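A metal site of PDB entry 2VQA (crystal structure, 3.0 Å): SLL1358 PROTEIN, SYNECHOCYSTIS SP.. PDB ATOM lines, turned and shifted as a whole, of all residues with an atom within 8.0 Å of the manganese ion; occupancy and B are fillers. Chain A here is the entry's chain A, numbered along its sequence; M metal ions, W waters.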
ATOM      1  N   MET A  57      23.356   5.866  -7.372  1.00  0.00           N
ATOM      2  CA  MET A  57      24.726   6.237  -7.071  1.00  0.00           C
ATOM      3  C   MET A  57      25.289   5.358  -5.958  1.00  0.00           C
ATOM      4  O   MET A  57      24.541   4.938  -5.060  1.00  0.00           O
ATOM      5  CB  MET A  57      24.819   7.700  -6.661  1.00  0.00           C
ATOM      6  CG  MET A  57      26.210   8.098  -6.285  1.00  0.00           C
ATOM      7  SD  MET A  57      26.417   9.868  -6.066  1.00  0.00           S
ATOM      8  CE  MET A  57      26.293  10.424  -7.766  1.00  0.00           C
ATOM      9  N   ARG A  65      30.898  12.488  -2.742  1.00  0.00           N
ATOM     10  CA  ARG A  65      30.310  13.237  -3.845  1.00  0.00           C
ATOM     11  C   ARG A  65      30.455  14.690  -3.385  1.00  0.00           C
ATOM     12  O   ARG A  65      29.784  15.126  -2.443  1.00  0.00           O
ATOM     13  CB  ARG A  65      28.853  12.787  -4.078  1.00  0.00           C
ATOM     14  CG  ARG A  65      27.882  13.715  -4.842  1.00  0.00           C
ATOM     15  CD  ARG A  65      27.909  13.626  -6.393  1.00  0.00           C
ATOM     16  NE  ARG A  65      28.557  14.826  -6.931  1.00  0.00           N
ATOM     17  CZ  ARG A  65      28.005  15.728  -7.743  1.00  0.00           C
ATOM     18  NH1 ARG A  65      26.763  15.578  -8.199  1.00  0.00           N
ATOM     19  NH2 ARG A  65      28.733  16.778  -8.133  1.00  0.00           N
ATOM     20  N   GLU A  66      31.389  15.399  -4.008  1.00  0.00           N
ATOM     21  CA  GLU A  66      31.828  16.743  -3.587  1.00  0.00           C
ATOM     22  C   GLU A  66      30.703  17.731  -3.311  1.00  0.00           C
ATOM     23  O   GLU A  66      29.582  17.570  -3.788  1.00  0.00           O
ATOM     24  CB  GLU A  66      32.736  17.354  -4.673  1.00  0.00           C
ATOM     25  CG  GLU A  66      32.015  17.679  -5.973  1.00  0.00           C
ATOM     26  CD  GLU A  66      32.752  18.699  -6.834  1.00  0.00           C
ATOM     27  OE1 GLU A  66      32.435  18.801  -8.044  1.00  0.00           O
ATOM     28  OE2 GLU A  66      33.639  19.403  -6.302  1.00  0.00           O
ATOM     29  N   LEU A  67      31.023  18.779  -2.549  1.00  0.00           N
ATOM     30  CA  LEU A  67      30.116  19.901  -2.309  1.00  0.00           C
ATOM     31  C   LEU A  67      29.535  20.510  -3.585  1.00  0.00           C
ATOM     32  O   LEU A  67      30.273  21.052  -4.426  1.00  0.00           O
ATOM     33  CB  LEU A  67      30.808  20.972  -1.472  1.00  0.00           C
ATOM     34  CG  LEU A  67      30.984  20.568  -0.004  1.00  0.00           C
ATOM     35  CD1 LEU A  67      32.013  21.430   0.669  1.00  0.00           C
ATOM     36  CD2 LEU A  67      29.686  20.621   0.792  1.00  0.00           C
ATOM     37  N   HIS A  68      28.218  20.410  -3.743  1.00  0.00           N
ATOM     38  CA  HIS A  68      27.539  20.868  -4.945  1.00  0.00           C
ATOM     39  C   HIS A  68      26.138  21.408  -4.634  1.00  0.00           C
ATOM     40  O   HIS A  68      25.638  21.246  -3.529  1.00  0.00           O
ATOM     41  CB  HIS A  68      27.511  19.747  -5.986  1.00  0.00           C
ATOM     42  CG  HIS A  68      26.509  18.662  -5.733  1.00  0.00           C
ATOM     43  ND1 HIS A  68      26.759  17.586  -4.901  1.00  0.00           N
ATOM     44  CD2 HIS A  68      25.273  18.438  -6.260  1.00  0.00           C
ATOM     45  CE1 HIS A  68      25.713  16.777  -4.896  1.00  0.00           C
ATOM     46  NE2 HIS A  68      24.804  17.273  -5.712  1.00  0.00           N
ATOM     47  N   TRP A  69      25.521  22.072  -5.603  1.00  0.00           N
ATOM     48  CA  TRP A  69      24.118  22.491  -5.476  1.00  0.00           C
ATOM     49  C   TRP A  69      23.395  22.406  -6.831  1.00  0.00           C
ATOM     50  O   TRP A  69      24.020  22.317  -7.876  1.00  0.00           O
ATOM     51  CB  TRP A  69      24.010  23.907  -4.883  1.00  0.00           C
ATOM     52  CG  TRP A  69      24.326  25.042  -5.831  1.00  0.00           C
ATOM     53  CD1 TRP A  69      23.439  25.729  -6.584  1.00  0.00           C
ATOM     54  CD2 TRP A  69      25.601  25.616  -6.098  1.00  0.00           C
ATOM     55  NE1 TRP A  69      24.071  26.698  -7.318  1.00  0.00           N
ATOM     56  CE2 TRP A  69      25.409  26.655  -7.028  1.00  0.00           C
ATOM     57  CE3 TRP A  69      26.902  25.347  -5.644  1.00  0.00           C
ATOM     58  CZ2 TRP A  69      26.438  27.422  -7.517  1.00  0.00           C
ATOM     59  CZ3 TRP A  69      27.928  26.122  -6.127  1.00  0.00           C
ATOM     60  CH2 TRP A  69      27.698  27.136  -7.056  1.00  0.00           C
ATOM     61  N   HIS A  70      22.077  22.421  -6.783  1.00  0.00           N
ATOM     62  CA  HIS A  70      21.297  22.508  -7.996  1.00  0.00           C
ATOM     63  C   HIS A  70      19.970  23.165  -7.673  1.00  0.00           C
ATOM     64  O   HIS A  70      19.140  22.596  -6.953  1.00  0.00           O
ATOM     65  CB  HIS A  70      21.086  21.111  -8.611  1.00  0.00           C
ATOM     66  CG  HIS A  70      21.098  19.991  -7.613  1.00  0.00           C
ATOM     67  ND1 HIS A  70      20.065  19.737  -6.745  1.00  0.00           N
ATOM     68  CD2 HIS A  70      22.028  19.033  -7.376  1.00  0.00           C
ATOM     69  CE1 HIS A  70      20.360  18.698  -5.995  1.00  0.00           C
ATOM     70  NE2 HIS A  70      21.545  18.235  -6.361  1.00  0.00           N
ATOM     71  N   ALA A  73      16.188  21.713  -8.983  1.00  0.00           N
ATOM     72  CA  ALA A  73      15.612  20.468  -8.460  1.00  0.00           C
ATOM     73  C   ALA A  73      15.884  20.157  -6.972  1.00  0.00           C
ATOM     74  O   ALA A  73      16.991  20.371  -6.468  1.00  0.00           O
ATOM     75  CB  ALA A  73      16.046  19.281  -9.307  1.00  0.00           C
ATOM     76  N   ALA A  74      14.853  19.631  -6.306  1.00  0.00           N
ATOM     77  CA  ALA A  74      14.972  19.096  -4.962  1.00  0.00           C
ATOM     78  C   ALA A  74      15.377  17.618  -5.005  1.00  0.00           C
ATOM     79  O   ALA A  74      15.032  16.886  -5.943  1.00  0.00           O
ATOM     80  CB  ALA A  74      13.669  19.250  -4.252  1.00  0.00           C
ATOM     81  N   GLU A  75      16.105  17.181  -3.984  1.00  0.00           N
ATOM     82  CA  GLU A  75      16.713  15.849  -3.966  1.00  0.00           C
ATOM     83  C   GLU A  75      16.154  15.089  -2.776  1.00  0.00           C
ATOM     84  O   GLU A  75      16.365  15.484  -1.635  1.00  0.00           O
ATOM     85  CB  GLU A  75      18.241  15.989  -3.892  1.00  0.00           C
ATOM     86  CG  GLU A  75      19.078  14.719  -3.964  1.00  0.00           C
ATOM     87  CD  GLU A  75      20.591  15.004  -3.918  1.00  0.00           C
ATOM     88  OE1 GLU A  75      21.065  15.889  -4.674  1.00  0.00           O
ATOM     89  OE2 GLU A  75      21.321  14.362  -3.137  1.00  0.00           O
ATOM     90  N   TRP A 106      16.986  11.199   2.900  1.00  0.00           N
ATOM     91  CA  TRP A 106      17.321  12.614   3.096  1.00  0.00           C
ATOM     92  C   TRP A 106      16.616  13.469   2.076  1.00  0.00           C
ATOM     93  O   TRP A 106      16.245  12.996   1.007  1.00  0.00           O
ATOM     94  CB  TRP A 106      18.836  12.879   3.101  1.00  0.00           C
ATOM     95  CG  TRP A 106      19.565  12.719   1.781  1.00  0.00           C
ATOM     96  CD1 TRP A 106      19.466  13.534   0.673  1.00  0.00           C
ATOM     97  CD2 TRP A 106      20.527  11.720   1.453  1.00  0.00           C
ATOM     98  NE1 TRP A 106      20.298  13.073  -0.322  1.00  0.00           N
ATOM     99  CE2 TRP A 106      20.962  11.960   0.132  1.00  0.00           C
ATOM    100  CE3 TRP A 106      21.059  10.622   2.158  1.00  0.00           C
ATOM    101  CZ2 TRP A 106      21.906  11.145  -0.501  1.00  0.00           C
ATOM    102  CZ3 TRP A 106      21.991   9.820   1.520  1.00  0.00           C
ATOM    103  CH2 TRP A 106      22.403  10.078   0.199  1.00  0.00           C
ATOM    104  N   PHE A 108      17.090  17.281   0.240  1.00  0.00           N
ATOM    105  CA  PHE A 108      17.848  18.490   0.029  1.00  0.00           C
ATOM    106  C   PHE A 108      17.018  19.526  -0.735  1.00  0.00           C
ATOM    107  O   PHE A 108      16.816  19.389  -1.941  1.00  0.00           O
ATOM    108  CB  PHE A 108      19.101  18.161  -0.761  1.00  0.00           C
ATOM    109  CG  PHE A 108      20.050  17.231  -0.038  1.00  0.00           C
ATOM    110  CD1 PHE A 108      20.007  17.116   1.349  1.00  0.00           C
ATOM    111  CD2 PHE A 108      21.010  16.508  -0.752  1.00  0.00           C
ATOM    112  CE1 PHE A 108      20.904  16.275   2.019  1.00  0.00           C
ATOM    113  CE2 PHE A 108      21.905  15.680  -0.084  1.00  0.00           C
ATOM    114  CZ  PHE A 108      21.854  15.570   1.294  1.00  0.00           C
ATOM    115  N   TRP A 112      20.074  24.219  -2.135  1.00  0.00           N
ATOM    116  CA  TRP A 112      20.865  24.152  -0.892  1.00  0.00           C
ATOM    117  C   TRP A 112      22.158  23.387  -1.138  1.00  0.00           C
ATOM    118  O   TRP A 112      22.155  22.371  -1.812  1.00  0.00           O
ATOM    119  CB  TRP A 112      20.086  23.490   0.246  1.00  0.00           C
ATOM    120  CG  TRP A 112      18.900  24.292   0.726  1.00  0.00           C
ATOM    121  CD1 TRP A 112      18.188  25.212   0.012  1.00  0.00           C
ATOM    122  CD2 TRP A 112      18.273  24.208   2.018  1.00  0.00           C
ATOM    123  NE1 TRP A 112      17.170  25.724   0.794  1.00  0.00           N
ATOM    124  CE2 TRP A 112      17.194  25.111   2.015  1.00  0.00           C
ATOM    125  CE3 TRP A 112      18.529  23.459   3.172  1.00  0.00           C
ATOM    126  CZ2 TRP A 112      16.374  25.289   3.133  1.00  0.00           C
ATOM    127  CZ3 TRP A 112      17.699  23.637   4.288  1.00  0.00           C
ATOM    128  CH2 TRP A 112      16.637  24.544   4.252  1.00  0.00           C
ATOM    129  N   GLY A 113      23.272  23.885  -0.614  1.00  0.00           N
ATOM    130  CA  GLY A 113      24.529  23.184  -0.788  1.00  0.00           C
ATOM    131  C   GLY A 113      24.552  21.929   0.067  1.00  0.00           C
ATOM    132  O   GLY A 113      24.091  21.949   1.205  1.00  0.00           O
ATOM    133  N   HIS A 114      25.102  20.846  -0.492  1.00  0.00           N
ATOM    134  CA  HIS A 114      25.202  19.571   0.215  1.00  0.00           C
ATOM    135  C   HIS A 114      26.344  18.682  -0.287  1.00  0.00           C
ATOM    136  O   HIS A 114      26.921  18.940  -1.333  1.00  0.00           O
ATOM    137  CB  HIS A 114      23.907  18.805   0.059  1.00  0.00           C
ATOM    138  CG  HIS A 114      23.454  18.675  -1.363  1.00  0.00           C
ATOM    139  ND1 HIS A 114      22.826  19.688  -2.046  1.00  0.00           N
ATOM    140  CD2 HIS A 114      23.530  17.633  -2.227  1.00  0.00           C
ATOM    141  CE1 HIS A 114      22.533  19.280  -3.272  1.00  0.00           C
ATOM    142  NE2 HIS A 114      22.945  18.034  -3.399  1.00  0.00           N
ATOM    143  N   SER A 115      26.664  17.643   0.491  1.00  0.00           N
ATOM    144  CA  SER A 115      27.651  16.625   0.112  1.00  0.00           C
ATOM    145  C   SER A 115      27.176  15.255   0.587  1.00  0.00           C
ATOM    146  O   SER A 115      26.288  15.173   1.441  1.00  0.00           O
ATOM    147  CB  SER A 115      28.973  16.911   0.763  1.00  0.00           C
ATOM    148  OG  SER A 115      28.878  16.595   2.139  1.00  0.00           O
ATOM    149  N   ILE A 116      27.750  14.185   0.054  1.00  0.00           N
ATOM    150  CA  ILE A 116      27.426  12.832   0.535  1.00  0.00           C
ATOM    151  C   ILE A 116      28.704  12.026   0.561  1.00  0.00           C
ATOM    152  O   ILE A 116      29.389  11.911  -0.459  1.00  0.00           O
ATOM    153  CB  ILE A 116      26.478  12.056  -0.407  1.00  0.00           C
ATOM    154  CG1 ILE A 116      25.292  12.898  -0.855  1.00  0.00           C
ATOM    155  CG2 ILE A 116      26.032  10.759   0.257  1.00  0.00           C
ATOM    156  CD1 ILE A 116      24.616  12.380  -2.060  1.00  0.00           C
ATOM    157  N   LEU A 128      18.475   8.536  -5.701  1.00  0.00           N
ATOM    158  CA  LEU A 128      18.198   9.958  -5.598  1.00  0.00           C
ATOM    159  C   LEU A 128      17.103  10.288  -6.579  1.00  0.00           C
ATOM    160  O   LEU A 128      17.277  10.121  -7.778  1.00  0.00           O
ATOM    161  CB  LEU A 128      19.443  10.790  -5.894  1.00  0.00           C
ATOM    162  CG  LEU A 128      20.751  10.540  -5.119  1.00  0.00           C
ATOM    163  CD1 LEU A 128      21.903  11.192  -5.849  1.00  0.00           C
ATOM    164  CD2 LEU A 128      20.707  11.000  -3.674  1.00  0.00           C
ATOM    165  N   PHE A 130      14.530  13.194  -8.121  1.00  0.00           N
ATOM    166  CA  PHE A 130      14.572  14.640  -8.242  1.00  0.00           C
ATOM    167  C   PHE A 130      13.270  15.152  -8.798  1.00  0.00           C
ATOM    168  O   PHE A 130      12.739  14.546  -9.722  1.00  0.00           O
ATOM    169  CB  PHE A 130      15.710  15.047  -9.168  1.00  0.00           C
ATOM    170  CG  PHE A 130      17.058  14.739  -8.625  1.00  0.00           C
ATOM    171  CD1 PHE A 130      17.731  15.646  -7.869  1.00  0.00           C
ATOM    172  CD2 PHE A 130      17.635  13.519  -8.854  1.00  0.00           C
ATOM    173  CE1 PHE A 130      18.989  15.353  -7.350  1.00  0.00           C
ATOM    174  CE2 PHE A 130      18.899  13.217  -8.355  1.00  0.00           C
ATOM    175  CZ  PHE A 130      19.570  14.138  -7.601  1.00  0.00           C
ATOM    176  N   PHE A 135      16.479  16.383 -14.879  1.00  0.00           N
ATOM    177  CA  PHE A 135      17.663  16.558 -14.052  1.00  0.00           C
ATOM    178  C   PHE A 135      18.777  15.596 -14.435  1.00  0.00           C
ATOM    179  O   PHE A 135      18.511  14.413 -14.671  1.00  0.00           O
ATOM    180  CB  PHE A 135      17.339  16.375 -12.571  1.00  0.00           C
ATOM    181  CG  PHE A 135      18.560  16.418 -11.690  1.00  0.00           C
ATOM    182  CD1 PHE A 135      18.964  17.607 -11.113  1.00  0.00           C
ATOM    183  CD2 PHE A 135      19.319  15.271 -11.495  1.00  0.00           C
ATOM    184  CE1 PHE A 135      20.095  17.647 -10.334  1.00  0.00           C
ATOM    185  CE2 PHE A 135      20.443  15.302 -10.724  1.00  0.00           C
ATOM    186  CZ  PHE A 135      20.834  16.491 -10.136  1.00  0.00           C
ATOM    187  N   GLU A 137      22.916  14.343 -13.375  1.00  0.00           N
ATOM    188  CA  GLU A 137      24.039  14.477 -12.485  1.00  0.00           C
ATOM    189  C   GLU A 137      25.239  15.142 -13.161  1.00  0.00           C
ATOM    190  O   GLU A 137      26.269  15.343 -12.536  1.00  0.00           O
ATOM    191  CB  GLU A 137      24.404  13.134 -11.850  1.00  0.00           C
ATOM    192  CG  GLU A 137      25.173  13.280 -10.506  1.00  0.00           C
ATOM    193  CD  GLU A 137      24.242  13.353  -9.292  1.00  0.00           C
ATOM    194  OE1 GLU A 137      23.025  13.383  -9.514  1.00  0.00           O
ATOM    195  OE2 GLU A 137      24.704  13.371  -8.111  1.00  0.00           O
ATOM    196  N   THR A 140      25.115  19.594 -12.376  1.00  0.00           N
ATOM    197  CA  THR A 140      25.048  20.166 -11.037  1.00  0.00           C
ATOM    198  C   THR A 140      26.085  21.274 -10.911  1.00  0.00           C
ATOM    199  O   THR A 140      26.989  21.412 -11.731  1.00  0.00           O
ATOM    200  CB  THR A 140      25.200  19.100  -9.916  1.00  0.00           C
ATOM    201  OG1 THR A 140      26.561  18.668  -9.802  1.00  0.00           O
ATOM    202  CG2 THR A 140      24.321  17.898 -10.175  1.00  0.00           C
ATOM    203  N   PHE A 141      25.930  22.113  -9.896  1.00  0.00           N
ATOM    204  CA  PHE A 141      26.912  23.150  -9.666  1.00  0.00           C
ATOM    205  C   PHE A 141      27.940  22.659  -8.653  1.00  0.00           C
ATOM    206  O   PHE A 141      27.610  22.380  -7.492  1.00  0.00           O
ATOM    207  CB  PHE A 141      26.245  24.415  -9.207  1.00  0.00           C
ATOM    208  CG  PHE A 141      25.582  25.171 -10.301  1.00  0.00           C
ATOM    209  CD1 PHE A 141      26.088  26.386 -10.728  1.00  0.00           C
ATOM    210  CD2 PHE A 141      24.431  24.681 -10.900  1.00  0.00           C
ATOM    211  CE1 PHE A 141      25.455  27.092 -11.743  1.00  0.00           C
ATOM    212  CE2 PHE A 141      23.801  25.379 -11.921  1.00  0.00           C
ATOM    213  CZ  PHE A 141      24.316  26.589 -12.338  1.00  0.00           C
HETATM  214 MN    MN M   1      22.789  16.594  -5.219  1.00  0.00          MN
HETATM  215  O   HOH W   1      22.821  15.472  -7.111  1.00  0.00           O
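The manganese ion is bound by the side-chain carboxylate of Glu 75 (1.9 Å), a ring nitrogen (NE2) of His 68 (2.2 Å), water W1 (2.2 Å), a ring nitrogen (NE2) of His 114 (2.3 Å) and a ring nitrogen (NE2) of His 70 (2.4 Å). The manganese ion has five donor atoms within binding distance.
Four residues have an atom within 4 Å of the manganese ion: His 68, His 70, Glu 75 and His 114. The nearest printed residue that does not touch the manganese ion is Phe 130 (4.5 Å).
The backbone carbonyl oxygen of Ala 73 sits at hydrogen-bond distance from a ring nitrogen (ND1) of His 70 (3.2 Å). The backbone carbonyl oxygen (O) of Trp 112 is in hydrogen-bond range of a ring nitrogen (ND1) of His 114 (2.8 Å). The backbone carbonyl oxygen (O) of Glu 66 lies within hydrogen-bond range of a ring nitrogen (ND1) of His 68, 3.0 Å away. The backbone NH (N) of Phe 108 sits at hydrogen-bond distance from the backbone carbonyl oxygen (O) of Glu 75 (2.7 Å). The side-chain carboxylate of Glu 75 is in hydrogen-bond range of the indole nitrogen of Trp 106 (3.3 Å).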
